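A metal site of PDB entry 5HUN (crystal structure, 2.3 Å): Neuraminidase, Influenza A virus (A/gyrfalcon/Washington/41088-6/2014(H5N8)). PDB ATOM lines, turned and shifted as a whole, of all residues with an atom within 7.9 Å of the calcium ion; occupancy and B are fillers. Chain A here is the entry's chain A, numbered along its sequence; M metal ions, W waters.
O of Tyr 274 lies close to OD1 of Asn 223 (3.4 Å).
OD1 of Asp 222 lies within hydrogen-bond range of N of Trp 224, 2.8 Å away.
O of Thr 227 is in hydrogen-bond range of N of Asp 252 (3.1 Å).
OD1 of Asp 252 sits at hydrogen-bond distance from N of Val 276, at 3.0 Å.
NH1 of Arg 229 lies within salt-bridge range of OD1 of Asp 252 (3.6 Å).
The backbone NH (N) of Gly 275 lies close to the backbone carbonyl oxygen (O) of Thr 253, 3.4 Å away.
The backbone carbonyl oxygen (O) of Asp 252 sits at hydrogen-bond distance from the guanidinium group (NH1) of Arg 255 (3.1 Å).
N of Gly 226 is in hydrogen-bond range of OD1 of Asp 222 (2.9 Å).
Gly 273 touches the calcium ion (O to CA, 3.8 Å).
Gly 275 touches the calcium ion.
Of the 23 residues printed, 6 come within 4 Å of the calcium ion.
The calcium ion is bound by the backbone carbonyl oxygen of Asp 222 (2.2 Å), the backbone carbonyl oxygen of Tyr 274 (2.3 Å), the side-chain carboxylate of Asp 252 (2.4 Å), water W1 (2.4 Å) and the backbone carbonyl oxygen of Gly 226 (2.4 Å).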
ATOM      1  N   HIS A 203      24.548 -24.483   2.418  1.00  0.00           N
ATOM      2  CA  HIS A 203      23.411 -23.583   2.577  1.00  0.00           C
ATOM      3  C   HIS A 203      22.329 -23.903   1.561  1.00  0.00           C
ATOM      4  O   HIS A 203      22.631 -24.268   0.418  1.00  0.00           O
ATOM      5  CB  HIS A 203      23.844 -22.105   2.493  1.00  0.00           C
ATOM      6  CG  HIS A 203      22.858 -21.137   3.101  1.00  0.00           C
ATOM      7  ND1 HIS A 203      22.202 -20.177   2.361  1.00  0.00           N
ATOM      8  CD2 HIS A 203      22.461 -20.952   4.381  1.00  0.00           C
ATOM      9  CE1 HIS A 203      21.441 -19.437   3.159  1.00  0.00           C
ATOM     10  NE2 HIS A 203      21.582 -19.892   4.396  1.00  0.00           N
ATOM     11  N   ARG A 221      19.494 -22.673  -3.845  1.00  0.00           N
ATOM     12  CA  ARG A 221      20.415 -21.536  -3.887  1.00  0.00           C
ATOM     13  C   ARG A 221      21.279 -21.535  -2.635  1.00  0.00           C
ATOM     14  O   ARG A 221      20.741 -21.600  -1.537  1.00  0.00           O
ATOM     15  CB  ARG A 221      19.625 -20.220  -3.996  1.00  0.00           C
ATOM     16  CG  ARG A 221      20.344 -18.937  -3.538  1.00  0.00           C
ATOM     17  CD  ARG A 221      19.341 -17.785  -3.457  1.00  0.00           C
ATOM     18  NE  ARG A 221      19.855 -16.553  -2.863  1.00  0.00           N
ATOM     19  CZ  ARG A 221      19.204 -15.386  -2.921  1.00  0.00           C
ATOM     20  NH1 ARG A 221      18.011 -15.295  -3.494  1.00  0.00           N
ATOM     21  NH2 ARG A 221      19.710 -14.319  -2.357  1.00  0.00           N
ATOM     22  N   ASP A 222      22.597 -21.455  -2.815  1.00  0.00           N
ATOM     23  CA  ASP A 222      23.530 -21.256  -1.718  1.00  0.00           C
ATOM     24  C   ASP A 222      23.836 -19.759  -1.548  1.00  0.00           C
ATOM     25  O   ASP A 222      24.441 -19.150  -2.448  1.00  0.00           O
ATOM     26  CB  ASP A 222      24.810 -22.043  -1.967  1.00  0.00           C
ATOM     27  CG  ASP A 222      25.820 -21.921  -0.826  1.00  0.00           C
ATOM     28  OD1 ASP A 222      26.173 -20.795  -0.430  1.00  0.00           O
ATOM     29  OD2 ASP A 222      26.327 -22.949  -0.360  1.00  0.00           O
ATOM     30  N   ASN A 223      23.474 -19.208  -0.387  1.00  0.00           N
ATOM     31  CA  ASN A 223      23.633 -17.791  -0.110  1.00  0.00           C
ATOM     32  C   ASN A 223      24.792 -17.495   0.816  1.00  0.00           C
ATOM     33  O   ASN A 223      24.996 -16.354   1.201  1.00  0.00           O
ATOM     34  CB  ASN A 223      22.338 -17.199   0.480  1.00  0.00           C
ATOM     35  CG  ASN A 223      22.085 -15.767  -0.007  1.00  0.00           C
ATOM     36  OD1 ASN A 223      21.861 -15.528  -1.205  1.00  0.00           O
ATOM     37  ND2 ASN A 223      22.171 -14.811   0.908  1.00  0.00           N
ATOM     38  N   TRP A 224      25.576 -18.526   1.141  1.00  0.00           N
ATOM     39  CA  TRP A 224      26.695 -18.448   2.053  1.00  0.00           C
ATOM     40  C   TRP A 224      28.000 -18.352   1.223  1.00  0.00           C
ATOM     41  O   TRP A 224      28.453 -17.267   0.881  1.00  0.00           O
ATOM     42  CB  TRP A 224      26.625 -19.664   3.004  1.00  0.00           C
ATOM     43  CG  TRP A 224      27.630 -19.676   4.173  1.00  0.00           C
ATOM     44  CD1 TRP A 224      28.506 -18.683   4.524  1.00  0.00           C
ATOM     45  CD2 TRP A 224      27.841 -20.728   5.124  1.00  0.00           C
ATOM     46  NE1 TRP A 224      29.253 -19.054   5.601  1.00  0.00           N
ATOM     47  CE2 TRP A 224      28.874 -20.298   6.011  1.00  0.00           C
ATOM     48  CE3 TRP A 224      27.270 -21.986   5.329  1.00  0.00           C
ATOM     49  CZ2 TRP A 224      29.344 -21.076   7.086  1.00  0.00           C
ATOM     50  CZ3 TRP A 224      27.746 -22.786   6.409  1.00  0.00           C
ATOM     51  CH2 TRP A 224      28.771 -22.311   7.274  1.00  0.00           C
ATOM     52  N   THR A 225      28.600 -19.471   0.848  1.00  0.00           N
ATOM     53  CA  THR A 225      29.870 -19.406   0.160  1.00  0.00           C
ATOM     54  C   THR A 225      29.846 -19.941  -1.294  1.00  0.00           C
ATOM     55  O   THR A 225      30.842 -19.811  -2.021  1.00  0.00           O
ATOM     56  CB  THR A 225      30.933 -20.200   0.946  1.00  0.00           C
ATOM     57  OG1 THR A 225      30.667 -21.605   0.826  1.00  0.00           O
ATOM     58  CG2 THR A 225      30.936 -19.795   2.468  1.00  0.00           C
ATOM     59  N   GLY A 226      28.736 -20.536  -1.722  1.00  0.00           N
ATOM     60  CA  GLY A 226      28.737 -21.278  -2.985  1.00  0.00           C
ATOM     61  C   GLY A 226      28.153 -20.507  -4.154  1.00  0.00           C
ATOM     62  O   GLY A 226      27.039 -19.991  -4.057  1.00  0.00           O
ATOM     63  N   THR A 227      28.937 -20.415  -5.233  1.00  0.00           N
ATOM     64  CA  THR A 227      28.470 -19.963  -6.551  1.00  0.00           C
ATOM     65  C   THR A 227      27.944 -21.149  -7.373  1.00  0.00           C
ATOM     66  O   THR A 227      27.446 -20.960  -8.483  1.00  0.00           O
ATOM     67  CB  THR A 227      29.601 -19.362  -7.402  1.00  0.00           C
ATOM     68  OG1 THR A 227      30.554 -20.372  -7.684  1.00  0.00           O
ATOM     69  CG2 THR A 227      30.295 -18.229  -6.702  1.00  0.00           C
ATOM     70  N   ASN A 228      28.105 -22.374  -6.852  1.00  0.00           N
ATOM     71  CA  ASN A 228      27.357 -23.501  -7.353  1.00  0.00           C
ATOM     72  C   ASN A 228      26.090 -23.703  -6.521  1.00  0.00           C
ATOM     73  O   ASN A 228      25.945 -23.199  -5.404  1.00  0.00           O
ATOM     74  CB  ASN A 228      28.164 -24.812  -7.405  1.00  0.00           C
ATOM     75  CG  ASN A 228      28.814 -25.185  -6.067  1.00  0.00           C
ATOM     76  OD1 ASN A 228      28.904 -24.365  -5.151  1.00  0.00           O
ATOM     77  ND2 ASN A 228      29.289 -26.412  -5.954  1.00  0.00           N
ATOM     78  N   ARG A 229      25.193 -24.480  -7.108  1.00  0.00           N
ATOM     79  CA  ARG A 229      23.929 -24.767  -6.551  1.00  0.00           C
ATOM     80  C   ARG A 229      23.840 -26.123  -5.842  1.00  0.00           C
ATOM     81  O   ARG A 229      24.270 -27.148  -6.373  1.00  0.00           O
ATOM     82  CB  ARG A 229      22.947 -24.741  -7.706  1.00  0.00           C
ATOM     83  CG  ARG A 229      22.916 -23.389  -8.376  1.00  0.00           C
ATOM     84  CD  ARG A 229      21.637 -23.240  -9.145  1.00  0.00           C
ATOM     85  NE  ARG A 229      21.422 -21.852  -9.545  1.00  0.00           N
ATOM     86  CZ  ARG A 229      20.939 -20.916  -8.752  1.00  0.00           C
ATOM     87  NH1 ARG A 229      20.753 -19.684  -9.207  1.00  0.00           N
ATOM     88  NH2 ARG A 229      20.633 -21.221  -7.489  1.00  0.00           N
ATOM     89  N   PRO A 230      23.241 -26.148  -4.657  1.00  0.00           N
ATOM     90  CA  PRO A 230      23.043 -27.407  -3.998  1.00  0.00           C
ATOM     91  C   PRO A 230      21.975 -28.224  -4.704  1.00  0.00           C
ATOM     92  O   PRO A 230      21.105 -27.679  -5.353  1.00  0.00           O
ATOM     93  CB  PRO A 230      22.555 -27.016  -2.585  1.00  0.00           C
ATOM     94  CG  PRO A 230      22.710 -25.545  -2.474  1.00  0.00           C
ATOM     95  CD  PRO A 230      22.695 -25.025  -3.877  1.00  0.00           C
ATOM     96  N   ASP A 252      25.059 -19.949 -10.153  1.00  0.00           N
ATOM     97  CA  ASP A 252      24.494 -18.915  -9.256  1.00  0.00           C
ATOM     98  C   ASP A 252      24.882 -17.547  -9.829  1.00  0.00           C
ATOM     99  O   ASP A 252      25.630 -17.434 -10.802  1.00  0.00           O
ATOM    100  CB  ASP A 252      25.043 -19.089  -7.827  1.00  0.00           C
ATOM    101  CG  ASP A 252      24.104 -18.567  -6.752  1.00  0.00           C
ATOM    102  OD1 ASP A 252      23.054 -17.986  -7.100  1.00  0.00           O
ATOM    103  OD2 ASP A 252      24.408 -18.758  -5.538  1.00  0.00           O
ATOM    104  N   THR A 253      24.352 -16.503  -9.231  1.00  0.00           N
ATOM    105  CA  THR A 253      24.754 -15.151  -9.516  1.00  0.00           C
ATOM    106  C   THR A 253      24.759 -14.463  -8.153  1.00  0.00           C
ATOM    107  O   THR A 253      23.756 -14.517  -7.468  1.00  0.00           O
ATOM    108  CB  THR A 253      23.787 -14.417 -10.472  1.00  0.00           C
ATOM    109  OG1 THR A 253      23.630 -15.183 -11.691  1.00  0.00           O
ATOM    110  CG2 THR A 253      24.284 -13.022 -10.780  1.00  0.00           C
ATOM    111  N   PRO A 254      25.864 -13.803  -7.780  1.00  0.00           N
ATOM    112  CA  PRO A 254      27.083 -13.596  -8.548  1.00  0.00           C
ATOM    113  C   PRO A 254      27.932 -14.847  -8.598  1.00  0.00           C
ATOM    114  O   PRO A 254      27.784 -15.744  -7.757  1.00  0.00           O
ATOM    115  CB  PRO A 254      27.814 -12.527  -7.751  1.00  0.00           C
ATOM    116  CG  PRO A 254      27.407 -12.790  -6.341  1.00  0.00           C
ATOM    117  CD  PRO A 254      25.927 -13.102  -6.474  1.00  0.00           C
ATOM    118  N   ARG A 255      28.806 -14.919  -9.574  1.00  0.00           N
ATOM    119  CA  ARG A 255      29.722 -16.054  -9.681  1.00  0.00           C
ATOM    120  C   ARG A 255      31.040 -15.595 -10.259  1.00  0.00           C
ATOM    121  O   ARG A 255      31.168 -14.451 -10.674  1.00  0.00           O
ATOM    122  CB  ARG A 255      29.124 -17.144 -10.548  1.00  0.00           C
ATOM    123  CG  ARG A 255      28.846 -16.656 -11.952  1.00  0.00           C
ATOM    124  CD  ARG A 255      28.211 -17.724 -12.790  1.00  0.00           C
ATOM    125  NE  ARG A 255      27.962 -17.162 -14.108  1.00  0.00           N
ATOM    126  CZ  ARG A 255      26.841 -16.591 -14.527  1.00  0.00           C
ATOM    127  NH1 ARG A 255      25.761 -16.496 -13.712  1.00  0.00           N
ATOM    128  NH2 ARG A 255      26.784 -16.121 -15.765  1.00  0.00           N
ATOM    129  N   PRO A 268      30.321 -26.564  -1.605  1.00  0.00           N
ATOM    130  CA  PRO A 268      30.167 -25.330  -2.336  1.00  0.00           C
ATOM    131  C   PRO A 268      31.551 -24.914  -2.817  1.00  0.00           C
ATOM    132  O   PRO A 268      32.552 -25.112  -2.121  1.00  0.00           O
ATOM    133  CB  PRO A 268      29.638 -24.339  -1.285  1.00  0.00           C
ATOM    134  CG  PRO A 268      30.109 -24.866   0.042  1.00  0.00           C
ATOM    135  CD  PRO A 268      30.378 -26.354  -0.132  1.00  0.00           C
ATOM    136  N   MET A 269      31.568 -24.289  -3.978  1.00  0.00           N
ATOM    137  CA  MET A 269      32.799 -23.824  -4.574  1.00  0.00           C
ATOM    138  C   MET A 269      32.585 -22.394  -5.001  1.00  0.00           C
ATOM    139  O   MET A 269      31.438 -21.920  -5.071  1.00  0.00           O
ATOM    140  CB  MET A 269      33.176 -24.694  -5.784  1.00  0.00           C
ATOM    141  CG  MET A 269      33.347 -26.173  -5.466  1.00  0.00           C
ATOM    142  SD  MET A 269      34.760 -26.480  -4.380  1.00  0.00           S
ATOM    143  CE  MET A 269      36.088 -25.888  -5.416  1.00  0.00           C
ATOM    144  N   ASN A 271      33.525 -19.547  -3.450  1.00  0.00           N
ATOM    145  CA  ASN A 271      33.766 -18.650  -2.336  1.00  0.00           C
ATOM    146  C   ASN A 271      33.338 -17.217  -2.584  1.00  0.00           C
ATOM    147  O   ASN A 271      34.135 -16.282  -2.535  1.00  0.00           O
ATOM    148  CB  ASN A 271      35.228 -18.710  -1.896  1.00  0.00           C
ATOM    149  CG  ASN A 271      35.601 -20.085  -1.386  1.00  0.00           C
ATOM    150  OD1 ASN A 271      35.840 -21.007  -2.172  1.00  0.00           O
ATOM    151  ND2 ASN A 271      35.663 -20.242  -0.053  1.00  0.00           N
ATOM    152  N   GLN A 272      32.051 -17.055  -2.866  1.00  0.00           N
ATOM    153  CA  GLN A 272      31.382 -15.746  -2.885  1.00  0.00           C
ATOM    154  C   GLN A 272      30.027 -15.920  -2.208  1.00  0.00           C
ATOM    155  O   GLN A 272      29.457 -16.999  -2.264  1.00  0.00           O
ATOM    156  CB  GLN A 272      31.149 -15.252  -4.319  1.00  0.00           C
ATOM    157  CG  GLN A 272      32.384 -15.164  -5.219  1.00  0.00           C
ATOM    158  CD  GLN A 272      32.025 -14.662  -6.608  1.00  0.00           C
ATOM    159  OE1 GLN A 272      32.389 -15.277  -7.625  1.00  0.00           O
ATOM    160  NE2 GLN A 272      31.307 -13.547  -6.677  1.00  0.00           N
ATOM    161  N   GLY A 273      29.551 -14.861  -1.554  1.00  0.00           N
ATOM    162  CA  GLY A 273      28.227 -14.825  -0.950  1.00  0.00           C
ATOM    163  C   GLY A 273      27.149 -14.487  -1.978  1.00  0.00           C
ATOM    164  O   GLY A 273      27.354 -14.633  -3.203  1.00  0.00           O
ATOM    165  N   TYR A 274      26.018 -13.998  -1.461  1.00  0.00           N
ATOM    166  CA  TYR A 274      24.846 -13.661  -2.273  1.00  0.00           C
ATOM    167  C   TYR A 274      24.372 -14.832  -3.138  1.00  0.00           C
ATOM    168  O   TYR A 274      24.793 -15.980  -2.948  1.00  0.00           O
ATOM    169  CB  TYR A 274      25.084 -12.415  -3.105  1.00  0.00           C
ATOM    170  CG  TYR A 274      25.797 -11.308  -2.372  1.00  0.00           C
ATOM    171  CD1 TYR A 274      25.239 -10.727  -1.233  1.00  0.00           C
ATOM    172  CD2 TYR A 274      27.021 -10.831  -2.820  1.00  0.00           C
ATOM    173  CE1 TYR A 274      25.899  -9.708  -0.555  1.00  0.00           C
ATOM    174  CE2 TYR A 274      27.694  -9.816  -2.160  1.00  0.00           C
ATOM    175  CZ  TYR A 274      27.130  -9.254  -1.020  1.00  0.00           C
ATOM    176  OH  TYR A 274      27.798  -8.228  -0.378  1.00  0.00           O
ATOM    177  N   GLY A 275      23.455 -14.554  -4.078  1.00  0.00           N
ATOM    178  CA  GLY A 275      22.726 -15.614  -4.754  1.00  0.00           C
ATOM    179  C   GLY A 275      21.454 -15.163  -5.464  1.00  0.00           C
ATOM    180  O   GLY A 275      20.963 -14.025  -5.308  1.00  0.00           O
ATOM    181  N   VAL A 276      20.910 -16.071  -6.264  1.00  0.00           N
ATOM    182  CA  VAL A 276      19.619 -15.855  -6.833  1.00  0.00           C
ATOM    183  C   VAL A 276      18.948 -17.206  -6.948  1.00  0.00           C
ATOM    184  O   VAL A 276      19.632 -18.184  -7.165  1.00  0.00           O
ATOM    185  CB  VAL A 276      19.716 -15.118  -8.189  1.00  0.00           C
ATOM    186  CG1 VAL A 276      20.218 -16.038  -9.296  1.00  0.00           C
ATOM    187  CG2 VAL A 276      18.385 -14.523  -8.558  1.00  0.00           C
HETATM  188 CA    CA M   1      25.726 -17.968  -3.747  1.00  0.00          CA
HETATM  189  O   HOH W   1      26.845 -17.588  -1.643  1.00  0.00           O
